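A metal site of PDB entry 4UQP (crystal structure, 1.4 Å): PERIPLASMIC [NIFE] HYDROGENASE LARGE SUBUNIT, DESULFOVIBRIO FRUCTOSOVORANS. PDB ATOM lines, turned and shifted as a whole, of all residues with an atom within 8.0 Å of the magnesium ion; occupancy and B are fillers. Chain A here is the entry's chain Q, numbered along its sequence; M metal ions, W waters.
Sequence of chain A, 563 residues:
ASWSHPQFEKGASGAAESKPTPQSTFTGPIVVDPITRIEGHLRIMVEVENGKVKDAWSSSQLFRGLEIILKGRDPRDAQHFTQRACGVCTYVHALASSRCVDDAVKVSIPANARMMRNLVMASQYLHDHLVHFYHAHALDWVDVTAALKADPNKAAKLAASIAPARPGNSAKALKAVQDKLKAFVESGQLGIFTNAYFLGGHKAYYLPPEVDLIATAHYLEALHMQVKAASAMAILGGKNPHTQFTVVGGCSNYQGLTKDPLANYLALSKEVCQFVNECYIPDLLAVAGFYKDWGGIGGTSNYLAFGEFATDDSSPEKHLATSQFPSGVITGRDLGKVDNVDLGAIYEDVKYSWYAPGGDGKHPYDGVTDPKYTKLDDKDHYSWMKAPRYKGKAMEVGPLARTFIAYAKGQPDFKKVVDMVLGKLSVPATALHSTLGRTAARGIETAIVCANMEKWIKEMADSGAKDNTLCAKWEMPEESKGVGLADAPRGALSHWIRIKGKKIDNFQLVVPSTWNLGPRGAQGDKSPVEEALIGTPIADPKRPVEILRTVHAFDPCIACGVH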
ATOM      1  N   PHE A  63      13.274   9.246 -13.313  1.00  0.00           N
ATOM      2  CA  PHE A  63      12.682   7.908 -13.284  1.00  0.00           C
ATOM      3  C   PHE A  63      11.274   7.968 -12.724  1.00  0.00           C
ATOM      4  O   PHE A  63      11.070   8.626 -11.704  1.00  0.00           O
ATOM      5  CB  PHE A  63      13.539   6.979 -12.431  1.00  0.00           C
ATOM      6  CG  PHE A  63      13.031   5.561 -12.330  1.00  0.00           C
ATOM      7  CD1 PHE A  63      13.306   4.630 -13.335  1.00  0.00           C
ATOM      8  CD2 PHE A  63      12.246   5.138 -11.243  1.00  0.00           C
ATOM      9  CE1 PHE A  63      12.846   3.327 -13.247  1.00  0.00           C
ATOM     10  CE2 PHE A  63      11.773   3.830 -11.154  1.00  0.00           C
ATOM     11  CZ  PHE A  63      12.081   2.911 -12.153  1.00  0.00           C
ATOM     12  N   GLU A  67       6.877   0.160 -15.171  1.00  0.00           N
ATOM     13  CA  GLU A  67       6.955  -1.303 -15.183  1.00  0.00           C
ATOM     14  C   GLU A  67       6.744  -1.866 -13.759  1.00  0.00           C
ATOM     15  O   GLU A  67       6.095  -2.893 -13.566  1.00  0.00           O
ATOM     16  CB  GLU A  67       8.323  -1.743 -15.715  1.00  0.00           C
ATOM     17  CG  GLU A  67       8.510  -1.389 -17.196  1.00  0.00           C
ATOM     18  CD  GLU A  67       9.949  -1.276 -17.609  1.00  0.00           C
ATOM     19  OE1 GLU A  67      10.802  -1.024 -16.730  1.00  0.00           O
ATOM     20  OE2 GLU A  67      10.224  -1.384 -18.830  1.00  0.00           O
ATOM     21  N   GLU A 348      18.393  -5.921 -22.855  1.00  0.00           N
ATOM     22  CA  GLU A 348      18.792  -4.644 -22.276  1.00  0.00           C
ATOM     23  C   GLU A 348      19.825  -4.806 -21.202  1.00  0.00           C
ATOM     24  O   GLU A 348      19.750  -5.743 -20.379  1.00  0.00           O
ATOM     25  CB  GLU A 348      17.598  -3.911 -21.663  1.00  0.00           C
ATOM     26  CG  GLU A 348      16.528  -3.521 -22.670  1.00  0.00           C
ATOM     27  CD  GLU A 348      15.351  -2.870 -22.005  1.00  0.00           C
ATOM     28  OE1 GLU A 348      14.588  -3.592 -21.341  1.00  0.00           O
ATOM     29  OE2 GLU A 348      15.144  -1.645 -22.181  1.00  0.00           O
ATOM     30  N   TYR A 355      20.562   1.214 -12.084  1.00  0.00           N
ATOM     31  CA  TYR A 355      19.865   0.007 -11.655  1.00  0.00           C
ATOM     32  C   TYR A 355      20.840  -0.883 -10.904  1.00  0.00           C
ATOM     33  O   TYR A 355      22.062  -0.708 -11.001  1.00  0.00           O
ATOM     34  CB  TYR A 355      19.222  -0.738 -12.853  1.00  0.00           C
ATOM     35  CG  TYR A 355      18.174   0.132 -13.523  1.00  0.00           C
ATOM     36  CD1 TYR A 355      16.897   0.264 -12.987  1.00  0.00           C
ATOM     37  CD2 TYR A 355      18.496   0.867 -14.649  1.00  0.00           C
ATOM     38  CE1 TYR A 355      15.967   1.128 -13.557  1.00  0.00           C
ATOM     39  CE2 TYR A 355      17.589   1.730 -15.226  1.00  0.00           C
ATOM     40  CZ  TYR A 355      16.326   1.845 -14.684  1.00  0.00           C
ATOM     41  OH  TYR A 355      15.403   2.711 -15.247  1.00  0.00           O
ATOM     42  N   PRO A 364      13.605  -8.882 -22.805  1.00  0.00           N
ATOM     43  CA  PRO A 364      12.544  -8.192 -22.065  1.00  0.00           C
ATOM     44  C   PRO A 364      11.482  -9.086 -21.423  1.00  0.00           C
ATOM     45  O   PRO A 364      10.838  -8.672 -20.464  1.00  0.00           O
ATOM     46  CB  PRO A 364      11.942  -7.234 -23.112  1.00  0.00           C
ATOM     47  CG  PRO A 364      13.034  -7.046 -24.102  1.00  0.00           C
ATOM     48  CD  PRO A 364      13.748  -8.358 -24.179  1.00  0.00           C
ATOM     49  N   GLY A 367      12.880  -9.204 -18.167  1.00  0.00           N
ATOM     50  CA  GLY A 367      13.376  -7.916 -17.734  1.00  0.00           C
ATOM     51  C   GLY A 367      13.241  -7.676 -16.245  1.00  0.00           C
ATOM     52  O   GLY A 367      12.365  -8.193 -15.590  1.00  0.00           O
ATOM     53  N   VAL A 368      14.146  -6.840 -15.735  1.00  0.00           N
ATOM     54  CA  VAL A 368      14.186  -6.466 -14.333  1.00  0.00           C
ATOM     55  C   VAL A 368      14.364  -4.956 -14.245  1.00  0.00           C
ATOM     56  O   VAL A 368      15.178  -4.360 -14.994  1.00  0.00           O
ATOM     57  CB  VAL A 368      15.435  -7.103 -13.648  1.00  0.00           C
ATOM     58  CG1 VAL A 368      15.459  -6.783 -12.156  1.00  0.00           C
ATOM     59  CG2 VAL A 368      15.519  -8.603 -13.917  1.00  0.00           C
ATOM     60  N   THR A 369      13.611  -4.333 -13.330  1.00  0.00           N
ATOM     61  CA  THR A 369      13.647  -2.879 -13.168  1.00  0.00           C
ATOM     62  C   THR A 369      13.813  -2.580 -11.697  1.00  0.00           C
ATOM     63  O   THR A 369      12.837  -2.489 -10.956  1.00  0.00           O
ATOM     64  CB  THR A 369      12.403  -2.212 -13.781  1.00  0.00           C
ATOM     65  OG1 THR A 369      12.290  -2.647 -15.146  1.00  0.00           O
ATOM     66  CG2 THR A 369      12.512  -0.682 -13.746  1.00  0.00           C
ATOM     67  N   TRP A 384      19.114   7.020 -16.117  1.00  0.00           N
ATOM     68  CA  TRP A 384      17.950   6.213 -15.807  1.00  0.00           C
ATOM     69  C   TRP A 384      17.449   5.370 -16.973  1.00  0.00           C
ATOM     70  O   TRP A 384      16.585   4.519 -16.764  1.00  0.00           O
ATOM     71  CB  TRP A 384      16.815   7.104 -15.318  1.00  0.00           C
ATOM     72  CG  TRP A 384      17.019   7.623 -13.925  1.00  0.00           C
ATOM     73  CD1 TRP A 384      17.265   8.930 -13.565  1.00  0.00           C
ATOM     74  CD2 TRP A 384      17.011   6.859 -12.716  1.00  0.00           C
ATOM     75  NE1 TRP A 384      17.394   9.017 -12.179  1.00  0.00           N
ATOM     76  CE2 TRP A 384      17.253   7.762 -11.642  1.00  0.00           C
ATOM     77  CE3 TRP A 384      16.824   5.506 -12.435  1.00  0.00           C
ATOM     78  CZ2 TRP A 384      17.293   7.351 -10.314  1.00  0.00           C
ATOM     79  CZ3 TRP A 384      16.874   5.088 -11.115  1.00  0.00           C
ATOM     80  CH2 TRP A 384      17.094   6.006 -10.069  1.00  0.00           C
ATOM     81  N   MET A 385      17.958   5.571 -18.178  1.00  0.00           N
ATOM     82  CA  MET A 385      17.614   4.619 -19.249  1.00  0.00           C
ATOM     83  C   MET A 385      18.471   3.360 -19.153  1.00  0.00           C
ATOM     84  O   MET A 385      19.676   3.431 -18.820  1.00  0.00           O
ATOM     85  CB  MET A 385      17.833   5.224 -20.623  1.00  0.00           C
ATOM     86  CG  MET A 385      16.824   6.323 -20.953  1.00  0.00           C
ATOM     87  SD  MET A 385      16.915   6.649 -22.736  1.00  0.00           S
ATOM     88  CE  MET A 385      16.172   8.270 -22.844  1.00  0.00           C
ATOM     89  N   LYS A 386      17.832   2.226 -19.460  1.00  0.00           N
ATOM     90  CA  LYS A 386      18.587   1.007 -19.797  1.00  0.00           C
ATOM     91  C   LYS A 386      19.233   1.171 -21.172  1.00  0.00           C
ATOM     92  O   LYS A 386      18.972   2.150 -21.886  1.00  0.00           O
ATOM     93  CB  LYS A 386      17.645  -0.202 -19.789  1.00  0.00           C
ATOM     94  CG  LYS A 386      16.956  -0.433 -18.451  1.00  0.00           C
ATOM     95  CD  LYS A 386      16.097  -1.706 -18.478  1.00  0.00           C
ATOM     96  CE  LYS A 386      15.390  -1.933 -17.138  1.00  0.00           C
ATOM     97  NZ  LYS A 386      14.319  -2.967 -17.302  1.00  0.00           N
ATOM     98  N   PRO A 388      19.420  -0.792 -24.502  1.00  0.00           N
ATOM     99  CA  PRO A 388      18.997  -1.923 -25.350  1.00  0.00           C
ATOM    100  C   PRO A 388      20.048  -2.203 -26.428  1.00  0.00           C
ATOM    101  O   PRO A 388      20.615  -1.270 -27.004  1.00  0.00           O
ATOM    102  CB  PRO A 388      17.685  -1.419 -25.988  1.00  0.00           C
ATOM    103  CG  PRO A 388      17.321  -0.166 -25.228  1.00  0.00           C
ATOM    104  CD  PRO A 388      18.646   0.425 -24.817  1.00  0.00           C
ATOM    105  N   SER A 494       8.516  -1.743 -28.381  1.00  0.00           N
ATOM    106  CA  SER A 494       7.998  -3.051 -28.014  1.00  0.00           C
ATOM    107  C   SER A 494       7.592  -3.080 -26.545  1.00  0.00           C
ATOM    108  O   SER A 494       8.310  -2.545 -25.677  1.00  0.00           O
ATOM    109  CB  SER A 494       8.997  -4.179 -28.379  1.00  0.00           C
ATOM    110  OG  SER A 494      10.297  -3.958 -27.825  1.00  0.00           O
ATOM    111  N   TRP A 496       6.268  -5.989 -23.620  1.00  0.00           N
ATOM    112  CA  TRP A 496       6.410  -7.442 -23.394  1.00  0.00           C
ATOM    113  C   TRP A 496       5.772  -7.794 -22.055  1.00  0.00           C
ATOM    114  O   TRP A 496       6.149  -7.221 -21.043  1.00  0.00           O
ATOM    115  CB  TRP A 496       7.894  -7.800 -23.297  1.00  0.00           C
ATOM    116  CG  TRP A 496       8.758  -7.270 -24.440  1.00  0.00           C
ATOM    117  CD1 TRP A 496       9.177  -5.987 -24.627  1.00  0.00           C
ATOM    118  CD2 TRP A 496       9.298  -8.046 -25.529  1.00  0.00           C
ATOM    119  NE1 TRP A 496       9.944  -5.908 -25.777  1.00  0.00           N
ATOM    120  CE2 TRP A 496      10.056  -7.159 -26.327  1.00  0.00           C
ATOM    121  CE3 TRP A 496       9.237  -9.404 -25.870  1.00  0.00           C
ATOM    122  CZ2 TRP A 496      10.719  -7.577 -27.464  1.00  0.00           C
ATOM    123  CZ3 TRP A 496       9.922  -9.823 -27.044  1.00  0.00           C
ATOM    124  CH2 TRP A 496      10.658  -8.914 -27.798  1.00  0.00           C
ATOM    125  N   PHE A 507       5.926  -6.714 -16.898  1.00  0.00           N
ATOM    126  CA  PHE A 507       5.569  -5.896 -18.032  1.00  0.00           C
ATOM    127  C   PHE A 507       6.747  -5.001 -18.311  1.00  0.00           C
ATOM    128  O   PHE A 507       7.141  -4.223 -17.440  1.00  0.00           O
ATOM    129  CB  PHE A 507       4.282  -5.102 -17.767  1.00  0.00           C
ATOM    130  CG  PHE A 507       3.640  -4.605 -19.037  1.00  0.00           C
ATOM    131  CD1 PHE A 507       4.208  -3.566 -19.792  1.00  0.00           C
ATOM    132  CD2 PHE A 507       2.487  -5.236 -19.507  1.00  0.00           C
ATOM    133  CE1 PHE A 507       3.620  -3.150 -20.975  1.00  0.00           C
ATOM    134  CE2 PHE A 507       1.876  -4.797 -20.674  1.00  0.00           C
ATOM    135  CZ  PHE A 507       2.461  -3.763 -21.416  1.00  0.00           C
ATOM    136  N   GLN A 508       7.337  -5.124 -19.496  1.00  0.00           N
ATOM    137  CA  GLN A 508       8.568  -4.398 -19.833  1.00  0.00           C
ATOM    138  C   GLN A 508       8.373  -3.599 -21.096  1.00  0.00           C
ATOM    139  O   GLN A 508       7.879  -4.140 -22.102  1.00  0.00           O
ATOM    140  CB  GLN A 508       9.753  -5.362 -20.016  1.00  0.00           C
ATOM    141  CG  GLN A 508      10.156  -6.065 -18.716  1.00  0.00           C
ATOM    142  CD  GLN A 508      10.858  -5.149 -17.718  1.00  0.00           C
ATOM    143  OE1 GLN A 508      11.665  -4.299 -18.103  1.00  0.00           O
ATOM    144  NE2 GLN A 508      10.597  -5.360 -16.426  1.00  0.00           N
ATOM    145  N   LEU A 509       8.709  -2.317 -21.039  1.00  0.00           N
ATOM    146  CA  LEU A 509       8.720  -1.458 -22.223  1.00  0.00           C
ATOM    147  C   LEU A 509      10.158  -1.288 -22.698  1.00  0.00           C
ATOM    148  O   LEU A 509      11.054  -1.016 -21.898  1.00  0.00           O
ATOM    149  CB  LEU A 509       8.172  -0.045 -21.895  1.00  0.00           C
ATOM    150  CG  LEU A 509       6.705   0.086 -21.443  1.00  0.00           C
ATOM    151  CD1 LEU A 509       6.422  -0.385 -20.032  1.00  0.00           C
ATOM    152  CD2 LEU A 509       6.258   1.539 -21.564  1.00  0.00           C
ATOM    153  N   VAL A 510      10.370  -1.415 -24.008  1.00  0.00           N
ATOM    154  CA  VAL A 510      11.667  -1.097 -24.620  1.00  0.00           C
ATOM    155  C   VAL A 510      11.309  -0.089 -25.725  1.00  0.00           C
ATOM    156  O   VAL A 510      10.602  -0.434 -26.678  1.00  0.00           O
ATOM    157  CB  VAL A 510      12.372  -2.342 -25.203  1.00  0.00           C
ATOM    158  CG1 VAL A 510      13.759  -1.954 -25.723  1.00  0.00           C
ATOM    159  CG2 VAL A 510      12.465  -3.454 -24.161  1.00  0.00           C
ATOM    160  N   VAL A 511      11.773   1.139 -25.591  1.00  0.00           N
ATOM    161  CA  VAL A 511      11.167   2.259 -26.320  1.00  0.00           C
ATOM    162  C   VAL A 511      12.189   2.868 -27.268  1.00  0.00           C
ATOM    163  O   VAL A 511      13.402   2.765 -27.021  1.00  0.00           O
ATOM    164  CB  VAL A 511      10.619   3.258 -25.264  1.00  0.00           C
ATOM    165  CG1 VAL A 511       9.808   4.391 -25.863  1.00  0.00           C
ATOM    166  CG2 VAL A 511       9.728   2.523 -24.263  1.00  0.00           C
ATOM    167  N   THR A 514      14.917   4.809 -25.802  1.00  0.00           N
ATOM    168  CA  THR A 514      15.828   3.928 -25.063  1.00  0.00           C
ATOM    169  C   THR A 514      16.939   3.416 -25.982  1.00  0.00           C
ATOM    170  O   THR A 514      18.144   3.507 -25.642  1.00  0.00           O
ATOM    171  CB  THR A 514      15.102   2.739 -24.377  1.00  0.00           C
ATOM    172  OG1 THR A 514      13.785   3.117 -23.936  1.00  0.00           O
ATOM    173  CG2 THR A 514      15.924   2.217 -23.209  1.00  0.00           C
ATOM    174  N   CYS A 560       9.441   8.672 -22.440  1.00  0.00           N
ATOM    175  CA  CYS A 560       9.417   7.406 -23.212  1.00  0.00           C
ATOM    176  C   CYS A 560      10.605   6.520 -22.867  1.00  0.00           C
ATOM    177  O   CYS A 560      10.434   5.324 -22.624  1.00  0.00           O
ATOM    178  CB  CYS A 560       9.502   7.712 -24.705  1.00  0.00           C
ATOM    179  SG  CYS A 560       7.904   7.748 -25.519  1.00  0.00           S
ATOM    180  N   GLY A 561      11.814   7.083 -22.912  1.00  0.00           N
ATOM    181  CA  GLY A 561      13.018   6.251 -22.849  1.00  0.00           C
ATOM    182  C   GLY A 561      13.179   5.553 -21.510  1.00  0.00           C
ATOM    183  O   GLY A 561      13.650   4.421 -21.455  1.00  0.00           O
ATOM    184  N   VAL A 562      12.816   6.256 -20.432  1.00  0.00           N
ATOM    185  CA  VAL A 562      12.986   5.698 -19.073  1.00  0.00           C
ATOM    186  C   VAL A 562      11.733   5.028 -18.542  1.00  0.00           C
ATOM    187  O   VAL A 562      11.799   3.980 -17.871  1.00  0.00           O
ATOM    188  CB  VAL A 562      13.370   6.826 -18.053  1.00  0.00           C
ATOM    189  CG1 VAL A 562      13.456   6.276 -16.613  1.00  0.00           C
ATOM    190  CG2 VAL A 562      14.678   7.520 -18.445  1.00  0.00           C
ATOM    191  N   HIS A 563      10.572   5.642 -18.813  1.00  0.00           N
ATOM    192  CA  HIS A 563       9.297   5.155 -18.274  1.00  0.00           C
ATOM    193  C   HIS A 563       9.394   4.808 -16.776  1.00  0.00           C
ATOM    194  O   HIS A 563       8.859   3.777 -16.319  1.00  0.00           O
ATOM    195  CB  HIS A 563       8.660   4.032 -19.140  1.00  0.00           C
ATOM    196  CG  HIS A 563       9.625   3.006 -19.649  1.00  0.00           C
ATOM    197  ND1 HIS A 563      10.415   3.229 -20.751  1.00  0.00           N
ATOM    198  CD2 HIS A 563       9.972   1.795 -19.167  1.00  0.00           C
ATOM    199  CE1 HIS A 563      11.198   2.173 -20.948  1.00  0.00           C
ATOM    200  NE2 HIS A 563      10.943   1.280 -20.002  1.00  0.00           N
ATOM    201  OXT HIS A 563       9.963   5.635 -16.010  1.00  0.00           O
HETATM  202 MG    MG M   1      11.907  -0.682 -19.981  1.00  0.00          MG
HETATM  203  O   HOH W   1      12.651  -2.619 -19.949  1.00  0.00           O
HETATM  204  O   HOH W   2      12.881  -0.298 -18.188  1.00  0.00           O
HETATM  205  O   HOH W   3      13.549   0.018 -20.989  1.00  0.00           O
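Water W3 is bound to the magnesium ion (2.0 Å). The magnesium ion is bound by water W1. Water W2 is bound to the magnesium ion. The magnesium ion is bound by O of Leu 509 (2.1 Å). OE2 of Glu 67 binds the magnesium ion, 2.2 Å away. The magnesium ion is bound by a ring nitrogen (NE2) of His 563 (2.2 Å).
ND1 of His 563 is in hydrogen-bond range of O of Cys 560 (2.8 Å). OE1 of Gln 508 lies close to OE2 of Glu 67, at 3.3 Å. The side-chain carboxylate (OE1) of Glu 67 sits at hydrogen-bond distance from the side-chain hydroxyl (OG1) of Thr 369, 2.7 Å away.
Water W1 lies within hydrogen-bond range of OE1 of Glu 348 (2.6 Å), OE1 of Gln 508 (2.7 Å) and NZ of Lys 386 (3.1 Å). Water W2 bridges the side-chain carboxylate of Glu 67 and the side-chain amino group of Lys 386.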
